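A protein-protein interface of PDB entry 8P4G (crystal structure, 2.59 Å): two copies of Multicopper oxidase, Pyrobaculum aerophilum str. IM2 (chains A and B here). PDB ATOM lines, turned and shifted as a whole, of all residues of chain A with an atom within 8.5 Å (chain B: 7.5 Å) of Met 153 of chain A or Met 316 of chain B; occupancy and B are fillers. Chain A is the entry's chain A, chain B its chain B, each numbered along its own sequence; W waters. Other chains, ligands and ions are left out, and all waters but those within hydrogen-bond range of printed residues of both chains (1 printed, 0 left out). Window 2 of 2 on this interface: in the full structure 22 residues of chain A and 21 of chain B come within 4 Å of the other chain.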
ATOM      1  N   PRO A 150      22.713 -18.495  24.690  1.00  0.00           N
ATOM      2  CA  PRO A 150      22.821 -17.896  23.356  1.00  0.00           C
ATOM      3  C   PRO A 150      23.534 -18.826  22.387  1.00  0.00           C
ATOM      4  O   PRO A 150      24.536 -19.459  22.727  1.00  0.00           O
ATOM      5  CB  PRO A 150      23.631 -16.621  23.607  1.00  0.00           C
ATOM      6  CG  PRO A 150      24.460 -16.946  24.797  1.00  0.00           C
ATOM      7  CD  PRO A 150      23.619 -17.851  25.657  1.00  0.00           C
ATOM      8  N   THR A 151      22.997 -18.910  21.175  1.00  0.00           N
ATOM      9  CA  THR A 151      23.655 -19.597  20.075  1.00  0.00           C
ATOM     10  C   THR A 151      24.757 -18.715  19.498  1.00  0.00           C
ATOM     11  O   THR A 151      24.865 -17.534  19.836  1.00  0.00           O
ATOM     12  CB  THR A 151      22.625 -19.958  19.007  1.00  0.00           C
ATOM     13  OG1 THR A 151      22.103 -18.760  18.421  1.00  0.00           O
ATOM     14  CG2 THR A 151      21.484 -20.756  19.621  1.00  0.00           C
ATOM     15  N   PRO A 152      25.625 -19.271  18.642  1.00  0.00           N
ATOM     16  CA  PRO A 152      26.587 -18.411  17.931  1.00  0.00           C
ATOM     17  C   PRO A 152      25.927 -17.252  17.201  1.00  0.00           C
ATOM     18  O   PRO A 152      26.463 -16.137  17.208  1.00  0.00           O
ATOM     19  CB  PRO A 152      27.272 -19.385  16.966  1.00  0.00           C
ATOM     20  CG  PRO A 152      27.191 -20.697  17.649  1.00  0.00           C
ATOM     21  CD  PRO A 152      25.894 -20.703  18.413  1.00  0.00           C
ATOM     22  N   MET A 153      24.774 -17.489  16.568  1.00  0.00           N
ATOM     23  CA  MET A 153      24.072 -16.409  15.881  1.00  0.00           C
ATOM     24  C   MET A 153      23.545 -15.381  16.874  1.00  0.00           C
ATOM     25  O   MET A 153      23.574 -14.174  16.602  1.00  0.00           O
ATOM     26  CB  MET A 153      22.929 -16.985  15.043  1.00  0.00           C
ATOM     27  CG  MET A 153      22.143 -15.966  14.226  1.00  0.00           C
ATOM     28  SD  MET A 153      23.128 -15.070  13.008  1.00  0.00           S
ATOM     29  CE  MET A 153      21.901 -13.944  12.346  1.00  0.00           C
ATOM     30  N   GLU A 154      23.063 -15.838  18.032  1.00  0.00           N
ATOM     31  CA  GLU A 154      22.587 -14.911  19.052  1.00  0.00           C
ATOM     32  C   GLU A 154      23.733 -14.122  19.670  1.00  0.00           C
ATOM     33  O   GLU A 154      23.527 -12.999  20.141  1.00  0.00           O
ATOM     34  CB  GLU A 154      21.812 -15.665  20.129  1.00  0.00           C
ATOM     35  CG  GLU A 154      20.334 -15.827  19.820  1.00  0.00           C
ATOM     36  CD  GLU A 154      19.707 -16.989  20.558  1.00  0.00           C
ATOM     37  OE1 GLU A 154      20.446 -17.738  21.230  1.00  0.00           O
ATOM     38  OE2 GLU A 154      18.470 -17.143  20.482  1.00  0.00           O
ATOM     39  N   MET A 155      24.941 -14.688  19.682  1.00  0.00           N
ATOM     40  CA  MET A 155      26.089 -13.948  20.194  1.00  0.00           C
ATOM     41  C   MET A 155      26.481 -12.800  19.274  1.00  0.00           C
ATOM     42  O   MET A 155      27.165 -11.873  19.721  1.00  0.00           O
ATOM     43  CB  MET A 155      27.276 -14.891  20.400  1.00  0.00           C
ATOM     44  CG  MET A 155      28.365 -14.340  21.316  1.00  0.00           C
ATOM     45  SD  MET A 155      27.844 -14.118  23.030  1.00  0.00           S
ATOM     46  CE  MET A 155      27.683 -15.819  23.567  1.00  0.00           C
ATOM     47  N   ILE A 156      26.056 -12.835  18.013  1.00  0.00           N
ATOM     48  CA  ILE A 156      26.306 -11.748  17.073  1.00  0.00           C
ATOM     49  C   ILE A 156      25.197 -10.705  17.127  1.00  0.00           C
ATOM     50  O   ILE A 156      25.465  -9.502  17.091  1.00  0.00           O
ATOM     51  CB  ILE A 156      26.470 -12.315  15.649  1.00  0.00           C
ATOM     52  CG1 ILE A 156      27.674 -13.252  15.573  1.00  0.00           C
ATOM     53  CG2 ILE A 156      26.605 -11.186  14.637  1.00  0.00           C
ATOM     54  CD1 ILE A 156      28.999 -12.538  15.662  1.00  0.00           C
ATOM     55  N   ALA A 157      23.943 -11.148  17.213  1.00  0.00           N
ATOM     56  CA  ALA A 157      22.807 -10.240  17.121  1.00  0.00           C
ATOM     57  C   ALA A 157      22.316  -9.755  18.476  1.00  0.00           C
ATOM     58  O   ALA A 157      21.735  -8.667  18.562  1.00  0.00           O
ATOM     59  CB  ALA A 157      21.653 -10.917  16.378  1.00  0.00           C
ATOM     60  N   GLY A 158      22.534 -10.526  19.536  1.00  0.00           N
ATOM     61  CA  GLY A 158      22.010 -10.176  20.841  1.00  0.00           C
ATOM     62  C   GLY A 158      21.012 -11.196  21.344  1.00  0.00           C
ATOM     63  O   GLY A 158      20.295 -11.813  20.549  1.00  0.00           O
ATOM     64  N   PHE A 159      20.954 -11.384  22.659  1.00  0.00           N
ATOM     65  CA  PHE A 159      20.079 -12.382  23.266  1.00  0.00           C
ATOM     66  C   PHE A 159      18.747 -11.726  23.619  1.00  0.00           C
ATOM     67  O   PHE A 159      18.680 -10.884  24.519  1.00  0.00           O
ATOM     68  CB  PHE A 159      20.746 -12.989  24.497  1.00  0.00           C
ATOM     69  CG  PHE A 159      20.093 -14.246  24.984  1.00  0.00           C
ATOM     70  CD1 PHE A 159      19.338 -14.244  26.145  1.00  0.00           C
ATOM     71  CD2 PHE A 159      20.240 -15.432  24.283  1.00  0.00           C
ATOM     72  CE1 PHE A 159      18.739 -15.402  26.598  1.00  0.00           C
ATOM     73  CE2 PHE A 159      19.642 -16.595  24.729  1.00  0.00           C
ATOM     74  CZ  PHE A 159      18.890 -16.580  25.889  1.00  0.00           C
ATOM     75  N   HIS A 257      17.598  -5.391  11.748  1.00  0.00           N
ATOM     76  CA  HIS A 257      18.304  -6.561  12.252  1.00  0.00           C
ATOM     77  C   HIS A 257      19.340  -7.050  11.232  1.00  0.00           C
ATOM     78  O   HIS A 257      19.830  -6.293  10.388  1.00  0.00           O
ATOM     79  CB  HIS A 257      17.302  -7.667  12.600  1.00  0.00           C
ATOM     80  CG  HIS A 257      16.731  -7.567  13.976  1.00  0.00           C
ATOM     81  ND1 HIS A 257      15.796  -8.460  14.454  1.00  0.00           N
ATOM     82  CD2 HIS A 257      16.971  -6.696  14.986  1.00  0.00           C
ATOM     83  CE1 HIS A 257      15.475  -8.136  15.694  1.00  0.00           C
ATOM     84  NE2 HIS A 257      16.175  -7.071  16.041  1.00  0.00           N
ATOM     85  N   LEU A 258      19.676  -8.341  11.314  1.00  0.00           N
ATOM     86  CA  LEU A 258      20.711  -8.991  10.522  1.00  0.00           C
ATOM     87  C   LEU A 258      22.053  -8.279  10.655  1.00  0.00           C
ATOM     88  O   LEU A 258      22.644  -7.846   9.670  1.00  0.00           O
ATOM     89  CB  LEU A 258      20.300  -9.085   9.048  1.00  0.00           C
ATOM     90  CG  LEU A 258      20.279 -10.504   8.478  1.00  0.00           C
ATOM     91  CD1 LEU A 258      19.236 -11.369   9.178  1.00  0.00           C
ATOM     92  CD2 LEU A 258      20.041 -10.476   6.979  1.00  0.00           C
ATOM     93  N   GLU A 266      11.799 -14.705  15.770  1.00  0.00           N
ATOM     94  CA  GLU A 266      11.793 -14.371  17.190  1.00  0.00           C
ATOM     95  C   GLU A 266      10.432 -14.610  17.846  1.00  0.00           C
ATOM     96  O   GLU A 266       9.385 -14.370  17.242  1.00  0.00           O
ATOM     97  CB  GLU A 266      12.227 -12.916  17.397  1.00  0.00           C
ATOM     98  CG  GLU A 266      13.687 -12.651  17.059  1.00  0.00           C
ATOM     99  CD  GLU A 266      14.652 -13.363  17.997  1.00  0.00           C
ATOM    100  OE1 GLU A 266      14.296 -13.567  19.179  1.00  0.00           O
ATOM    101  OE2 GLU A 266      15.766 -13.717  17.553  1.00  0.00           O
ATOM    102  N   LEU A 313      30.804  -5.291  11.334  1.00  0.00           N
ATOM    103  CA  LEU A 313      30.862  -6.714  11.654  1.00  0.00           C
ATOM    104  C   LEU A 313      31.928  -7.323  10.752  1.00  0.00           C
ATOM    105  O   LEU A 313      31.689  -7.568   9.566  1.00  0.00           O
ATOM    106  CB  LEU A 313      29.505  -7.385  11.459  1.00  0.00           C
ATOM    107  CG  LEU A 313      29.492  -8.892  11.725  1.00  0.00           C
ATOM    108  CD1 LEU A 313      29.935  -9.184  13.151  1.00  0.00           C
ATOM    109  CD2 LEU A 313      28.120  -9.490  11.452  1.00  0.00           C
ATOM    110  N   GLY A 315      33.394 -10.250   9.726  1.00  0.00           N
ATOM    111  CA  GLY A 315      33.162 -11.678   9.742  1.00  0.00           C
ATOM    112  C   GLY A 315      32.353 -12.106  10.948  1.00  0.00           C
ATOM    113  O   GLY A 315      31.124 -12.002  10.955  1.00  0.00           O
ATOM    114  N   MET A 316      33.043 -12.590  11.979  1.00  0.00           N
ATOM    115  CA  MET A 316      32.410 -13.064  13.199  1.00  0.00           C
ATOM    116  C   MET A 316      32.643 -12.141  14.388  1.00  0.00           C
ATOM    117  O   MET A 316      32.174 -12.441  15.490  1.00  0.00           O
ATOM    118  CB  MET A 316      32.914 -14.473  13.530  1.00  0.00           C
ATOM    119  CG  MET A 316      31.869 -15.386  14.134  1.00  0.00           C
ATOM    120  SD  MET A 316      30.957 -16.241  12.840  1.00  0.00           S
ATOM    121  CE  MET A 316      32.160 -17.456  12.317  1.00  0.00           C
ATOM    122  N   GLN A 317      33.351 -11.030  14.198  1.00  0.00           N
ATOM    123  CA  GLN A 317      33.823 -10.197  15.298  1.00  0.00           C
ATOM    124  C   GLN A 317      33.357  -8.767  15.079  1.00  0.00           C
ATOM    125  O   GLN A 317      33.729  -8.138  14.082  1.00  0.00           O
ATOM    126  CB  GLN A 317      35.352 -10.251  15.399  1.00  0.00           C
ATOM    127  CG  GLN A 317      35.967  -9.255  16.374  1.00  0.00           C
ATOM    128  CD  GLN A 317      35.699  -9.610  17.821  1.00  0.00           C
ATOM    129  OE1 GLN A 317      36.209 -10.607  18.333  1.00  0.00           O
ATOM    130  NE2 GLN A 317      34.896  -8.792  18.494  1.00  0.00           N
ATOM    131  N   TRP A 318      32.541  -8.258  16.000  1.00  0.00           N
ATOM    132  CA  TRP A 318      32.176  -6.849  15.966  1.00  0.00           C
ATOM    133  C   TRP A 318      33.402  -5.996  16.260  1.00  0.00           C
ATOM    134  O   TRP A 318      34.153  -6.273  17.201  1.00  0.00           O
ATOM    135  CB  TRP A 318      31.072  -6.552  16.978  1.00  0.00           C
ATOM    136  CG  TRP A 318      29.710  -6.967  16.525  1.00  0.00           C
ATOM    137  CD1 TRP A 318      28.973  -8.016  16.992  1.00  0.00           C
ATOM    138  CD2 TRP A 318      28.926  -6.350  15.498  1.00  0.00           C
ATOM    139  NE1 TRP A 318      27.774  -8.083  16.326  1.00  0.00           N
ATOM    140  CE2 TRP A 318      27.721  -7.072  15.402  1.00  0.00           C
ATOM    141  CE3 TRP A 318      29.124  -5.253  14.653  1.00  0.00           C
ATOM    142  CZ2 TRP A 318      26.719  -6.734  14.495  1.00  0.00           C
ATOM    143  CZ3 TRP A 318      28.129  -4.920  13.752  1.00  0.00           C
ATOM    144  CH2 TRP A 318      26.941  -5.657  13.680  1.00  0.00           C
ATOM    145  N   MET A 352      23.690  -3.441  12.635  1.00  0.00           N
ATOM    146  CA  MET A 352      22.473  -3.345  13.426  1.00  0.00           C
ATOM    147  C   MET A 352      22.651  -2.226  14.445  1.00  0.00           C
ATOM    148  O   MET A 352      23.664  -1.519  14.451  1.00  0.00           O
ATOM    149  CB  MET A 352      22.135  -4.674  14.108  1.00  0.00           C
ATOM    150  CG  MET A 352      23.258  -5.259  14.939  1.00  0.00           C
ATOM    151  SD  MET A 352      22.718  -6.737  15.811  1.00  0.00           S
ATOM    152  CE  MET A 352      21.398  -6.050  16.808  1.00  0.00           C
ATOM    153  N   GLU A 427      25.888  -9.016  24.408  1.00  0.00           N
ATOM    154  CA  GLU A 427      26.439 -10.052  23.543  1.00  0.00           C
ATOM    155  C   GLU A 427      27.558  -9.496  22.673  1.00  0.00           C
ATOM    156  O   GLU A 427      28.564 -10.176  22.437  1.00  0.00           O
ATOM    157  CB  GLU A 427      25.337 -10.673  22.682  1.00  0.00           C
ATOM    158  CG  GLU A 427      24.516 -11.731  23.404  1.00  0.00           C
ATOM    159  CD  GLU A 427      23.673 -11.157  24.521  1.00  0.00           C
ATOM    160  OE1 GLU A 427      22.956 -10.165  24.276  1.00  0.00           O
ATOM    161  OE2 GLU A 427      23.738 -11.691  25.647  1.00  0.00           O
ATOM    162  N   HIS A 428      27.399  -8.262  22.186  1.00  0.00           N
ATOM    163  CA  HIS A 428      28.454  -7.640  21.393  1.00  0.00           C
ATOM    164  C   HIS A 428      29.681  -7.348  22.245  1.00  0.00           C
ATOM    165  O   HIS A 428      30.816  -7.571  21.805  1.00  0.00           O
ATOM    166  CB  HIS A 428      27.945  -6.351  20.747  1.00  0.00           C
ATOM    167  CG  HIS A 428      26.837  -6.561  19.763  1.00  0.00           C
ATOM    168  ND1 HIS A 428      26.223  -5.518  19.104  1.00  0.00           N
ATOM    169  CD2 HIS A 428      26.230  -7.690  19.329  1.00  0.00           C
ATOM    170  CE1 HIS A 428      25.286  -5.996  18.305  1.00  0.00           C
ATOM    171  NE2 HIS A 428      25.270  -7.311  18.423  1.00  0.00           N
ATOM    172  N   PRO B 152      31.993 -15.539  19.728  1.00  0.00           N
ATOM    173  CA  PRO B 152      31.145 -16.189  18.713  1.00  0.00           C
ATOM    174  C   PRO B 152      31.885 -17.229  17.890  1.00  0.00           C
ATOM    175  O   PRO B 152      31.341 -18.305  17.612  1.00  0.00           O
ATOM    176  CB  PRO B 152      30.682 -15.012  17.846  1.00  0.00           C
ATOM    177  CG  PRO B 152      30.703 -13.852  18.754  1.00  0.00           C
ATOM    178  CD  PRO B 152      31.835 -14.073  19.716  1.00  0.00           C
ATOM    179  N   MET B 153      33.129 -16.933  17.506  1.00  0.00           N
ATOM    180  CA  MET B 153      33.911 -17.882  16.721  1.00  0.00           C
ATOM    181  C   MET B 153      34.274 -19.118  17.536  1.00  0.00           C
ATOM    182  O   MET B 153      34.306 -20.233  17.001  1.00  0.00           O
ATOM    183  CB  MET B 153      35.170 -17.205  16.184  1.00  0.00           C
ATOM    184  CG  MET B 153      36.018 -18.103  15.304  1.00  0.00           C
ATOM    185  SD  MET B 153      35.107 -18.670  13.855  1.00  0.00           S
ATOM    186  CE  MET B 153      36.302 -19.764  13.093  1.00  0.00           C
ATOM    187  N   MET B 155      32.511 -20.535  19.812  1.00  0.00           N
ATOM    188  CA  MET B 155      31.355 -21.425  19.852  1.00  0.00           C
ATOM    189  C   MET B 155      31.163 -22.191  18.552  1.00  0.00           C
ATOM    190  O   MET B 155      30.369 -23.137  18.526  1.00  0.00           O
ATOM    191  CB  MET B 155      30.085 -20.641  20.180  1.00  0.00           C
ATOM    192  CG  MET B 155      29.829 -20.489  21.668  1.00  0.00           C
ATOM    193  SD  MET B 155      28.335 -19.539  21.979  1.00  0.00           S
ATOM    194  CE  MET B 155      28.668 -18.105  20.965  1.00  0.00           C
ATOM    195  N   ILE B 156      31.866 -21.816  17.486  1.00  0.00           N
ATOM    196  CA  ILE B 156      31.832 -22.568  16.236  1.00  0.00           C
ATOM    197  C   ILE B 156      32.893 -23.660  16.228  1.00  0.00           C
ATOM    198  O   ILE B 156      32.628 -24.792  15.816  1.00  0.00           O
ATOM    199  CB  ILE B 156      32.008 -21.610  15.041  1.00  0.00           C
ATOM    200  CG1 ILE B 156      30.871 -20.586  14.993  1.00  0.00           C
ATOM    201  CG2 ILE B 156      32.089 -22.390  13.736  1.00  0.00           C
ATOM    202  CD1 ILE B 156      29.539 -21.173  14.589  1.00  0.00           C
ATOM    203  N   LEU B 313      28.688 -27.564   8.406  1.00  0.00           N
ATOM    204  CA  LEU B 313      28.501 -26.253   9.023  1.00  0.00           C
ATOM    205  C   LEU B 313      27.648 -25.420   8.074  1.00  0.00           C
ATOM    206  O   LEU B 313      28.144 -24.894   7.074  1.00  0.00           O
ATOM    207  CB  LEU B 313      29.841 -25.582   9.307  1.00  0.00           C
ATOM    208  CG  LEU B 313      29.780 -24.170   9.895  1.00  0.00           C
ATOM    209  CD1 LEU B 313      29.014 -24.158  11.212  1.00  0.00           C
ATOM    210  CD2 LEU B 313      31.178 -23.600  10.080  1.00  0.00           C
ATOM    211  N   SER B 314      26.358 -25.304   8.386  1.00  0.00           N
ATOM    212  CA  SER B 314      25.430 -24.515   7.577  1.00  0.00           C
ATOM    213  C   SER B 314      25.455 -23.083   8.097  1.00  0.00           C
ATOM    214  O   SER B 314      24.685 -22.704   8.980  1.00  0.00           O
ATOM    215  CB  SER B 314      24.030 -25.112   7.621  1.00  0.00           C
ATOM    216  OG  SER B 314      24.012 -26.412   7.053  1.00  0.00           O
ATOM    217  N   GLY B 315      26.357 -22.279   7.536  1.00  0.00           N
ATOM    218  CA  GLY B 315      26.539 -20.904   7.961  1.00  0.00           C
ATOM    219  C   GLY B 315      27.041 -20.766   9.385  1.00  0.00           C
ATOM    220  O   GLY B 315      28.239 -20.899   9.645  1.00  0.00           O
ATOM    221  N   MET B 316      26.126 -20.503  10.316  1.00  0.00           N
ATOM    222  CA  MET B 316      26.463 -20.319  11.721  1.00  0.00           C
ATOM    223  C   MET B 316      26.035 -21.499  12.579  1.00  0.00           C
ATOM    224  O   MET B 316      26.262 -21.483  13.793  1.00  0.00           O
ATOM    225  CB  MET B 316      25.802 -19.041  12.256  1.00  0.00           C
ATOM    226  CG  MET B 316      26.617 -18.274  13.277  1.00  0.00           C
ATOM    227  SD  MET B 316      27.689 -17.062  12.495  1.00  0.00           S
ATOM    228  CE  MET B 316      26.505 -15.790  12.063  1.00  0.00           C
ATOM    229  N   GLN B 317      25.426 -22.520  11.980  1.00  0.00           N
ATOM    230  CA  GLN B 317      24.787 -23.601  12.716  1.00  0.00           C
ATOM    231  C   GLN B 317      25.327 -24.934  12.225  1.00  0.00           C
ATOM    232  O   GLN B 317      25.153 -25.281  11.052  1.00  0.00           O
ATOM    233  CB  GLN B 317      23.265 -23.543  12.550  1.00  0.00           C
ATOM    234  CG  GLN B 317      22.532 -24.745  13.103  1.00  0.00           C
ATOM    235  CD  GLN B 317      22.555 -24.785  14.614  1.00  0.00           C
ATOM    236  OE1 GLN B 317      21.945 -23.946  15.278  1.00  0.00           O
ATOM    237  NE2 GLN B 317      23.264 -25.763  15.168  1.00  0.00           N
ATOM    238  N   TRP B 318      25.981 -25.675  13.115  1.00  0.00           N
ATOM    239  CA  TRP B 318      26.385 -27.038  12.799  1.00  0.00           C
ATOM    240  C   TRP B 318      25.148 -27.915  12.652  1.00  0.00           C
ATOM    241  O   TRP B 318      24.230 -27.852  13.476  1.00  0.00           O
ATOM    242  CB  TRP B 318      27.304 -27.589  13.888  1.00  0.00           C
ATOM    243  CG  TRP B 318      28.713 -27.088  13.797  1.00  0.00           C
ATOM    244  CD1 TRP B 318      29.313 -26.177  14.614  1.00  0.00           C
ATOM    245  CD2 TRP B 318      29.703 -27.480  12.838  1.00  0.00           C
ATOM    246  NE1 TRP B 318      30.613 -25.971  14.221  1.00  0.00           N
ATOM    247  CE2 TRP B 318      30.877 -26.760  13.133  1.00  0.00           C
ATOM    248  CE3 TRP B 318      29.711 -28.367  11.758  1.00  0.00           C
ATOM    249  CZ2 TRP B 318      32.045 -26.900  12.388  1.00  0.00           C
ATOM    250  CZ3 TRP B 318      30.871 -28.505  11.020  1.00  0.00           C
ATOM    251  CH2 TRP B 318      32.022 -27.775  11.339  1.00  0.00           C
ATOM    252  N   THR B 319      25.118 -28.732  11.601  1.00  0.00           N
ATOM    253  CA  THR B 319      23.935 -29.509  11.268  1.00  0.00           C
ATOM    254  C   THR B 319      24.286 -30.978  11.084  1.00  0.00           C
ATOM    255  O   THR B 319      25.402 -31.330  10.693  1.00  0.00           O
ATOM    256  CB  THR B 319      23.252 -28.996   9.989  1.00  0.00           C
ATOM    257  OG1 THR B 319      24.129 -29.173   8.869  1.00  0.00           O
ATOM    258  CG2 THR B 319      22.886 -27.525  10.121  1.00  0.00           C
ATOM    259  N   GLY B 431      25.569 -25.227  20.482  1.00  0.00           N
ATOM    260  CA  GLY B 431      25.131 -24.517  19.294  1.00  0.00           C
ATOM    261  C   GLY B 431      23.952 -25.151  18.586  1.00  0.00           C
ATOM    262  O   GLY B 431      23.309 -24.488  17.767  1.00  0.00           O
HETATM  263  O   HOH W   1      23.727 -20.092  15.332  1.00  0.00           O
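SD of Met 316 of chain A lies close to SD of Met 316 of chain B (3.4 Å).
Water W1 lies within hydrogen-bond range of the backbone NH (N) of Met 153 of chain A (3.1 Å) and the backbone carbonyl oxygen (O) of Met 316 of chain B (3.3 Å).
N of Met 153 of chain A lies close to OG1 of Thr 151 of chain A (3.5 Å). The backbone carbonyl oxygen (O) of Ile 156 of chain A is in hydrogen-bond range of the indole nitrogen (NE1) of Trp 318 of chain A, 2.8 Å away. O of Ile 156 of chain A is in hydrogen-bond range of NE2 of His 428 of chain A (2.6 Å). O of Ile 156 of chain B sits at hydrogen-bond distance from NE1 of Trp 318 of chain B, 2.8 Å away. The backbone carbonyl oxygen (O) of Gly 431 of chain B sits close to the side-chain amide oxygen (OE1) of Gln 317 of chain B, at 2.9 Å.
O of Pro 150 of chain A touches SD of Met 155 of chain B (3.9 Å). CA of Pro 152 of chain A touches CE of Met 155 of chain B, 3.7 Å away. CB of Pro 152 of chain A touches CD1 of Ile 156 of chain B, 3.7 Å away. CB of Pro 152 of chain A touches CG of Met 316 of chain B, at 3.9 Å. Pro 152 of chain A touches Gly 431 of chain B. Met 316 of chain B touches Met 153 of chain A. Met 155 of chain A touches Met 155 of chain B (CB to CE, 3.5 Å). Ile 156 of chain A touches Pro 152 of chain B (CD1 to CB, 3.7 Å). Pro 152 of chain B touches Met 316 of chain A (CB to O, 3.8 Å). Met 316 of chain A touches Met 153 of chain B.
Pro 152 of chain A touches Ile 156 of chain B, and with the chains exchanged Ile 156 of chain A touches Pro 152 of chain B. Met 153 of chain A touches Met 316 of chain B, and with the chains exchanged Met 316 of chain A touches Met 153 of chain B. Met 155 of chain A touches its own counterpart, Met 155 of chain B. Met 316 of chain B touches its own counterpart, Met 316 of chain A. Positions printed for both chains: 152, 153, 155, 156, 313, 315, 316, 317 and 318. Of the 12 pairs that touch across the chains among the printed residues, 10 have their exchanged pair printed and touching as well.
Of the 12 printed residues of chain B, 6 touch a printed residue of chain A. Hydrophobic or aromatic side chains of chain B that line the printed part of chain A: Pro 152, Met 153, Met 155, Ile 156 and Met 316. Along chain B the printed residues that touch a printed residue of chain A span positions 152 to 431. Printed residues of chain A that touch a printed residue of chain B: Pro 150, Pro 152, Met 153, Met 155, Ile 156 and Met 316. Hydrophobic or aromatic side chains of chain A that line the printed part of chain B: Pro 152, Met 153, Met 155, Ile 156 and Met 316. Among the printed residues, 12 pairs touch across the chains. Among the printed residues, no Asp or Glu carboxylate lies within 4 Å of a Lys or Arg side-chain nitrogen of the other chain.
Of chain B, only Met 316 comes within 4 Å of Met 153 of chain A. Printed residues of chain B within 4 Å of Ile 156 of chain A: Pro 152. Leu 313 of chain A touches none of the printed residues of chain B. Of the printed residues of chain A, Met 153 of chain B touches Met 316 (3.5 Å). Of the printed residues of chain A, Ile 156 of chain B touches Pro 152. No residue of chain A comes within 4 Å of Gly 315 of chain B. Of chain A, only Pro 152, Met 153 and Met 316 come within 4 Å of Met 316 of chain B. Of the printed residues of chain A, Gly 431 of chain B touches Pro 152. The nearest printed residue of chain A that does not touch Ile 156 of chain B is Met 316 of chain A (4.3 Å).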
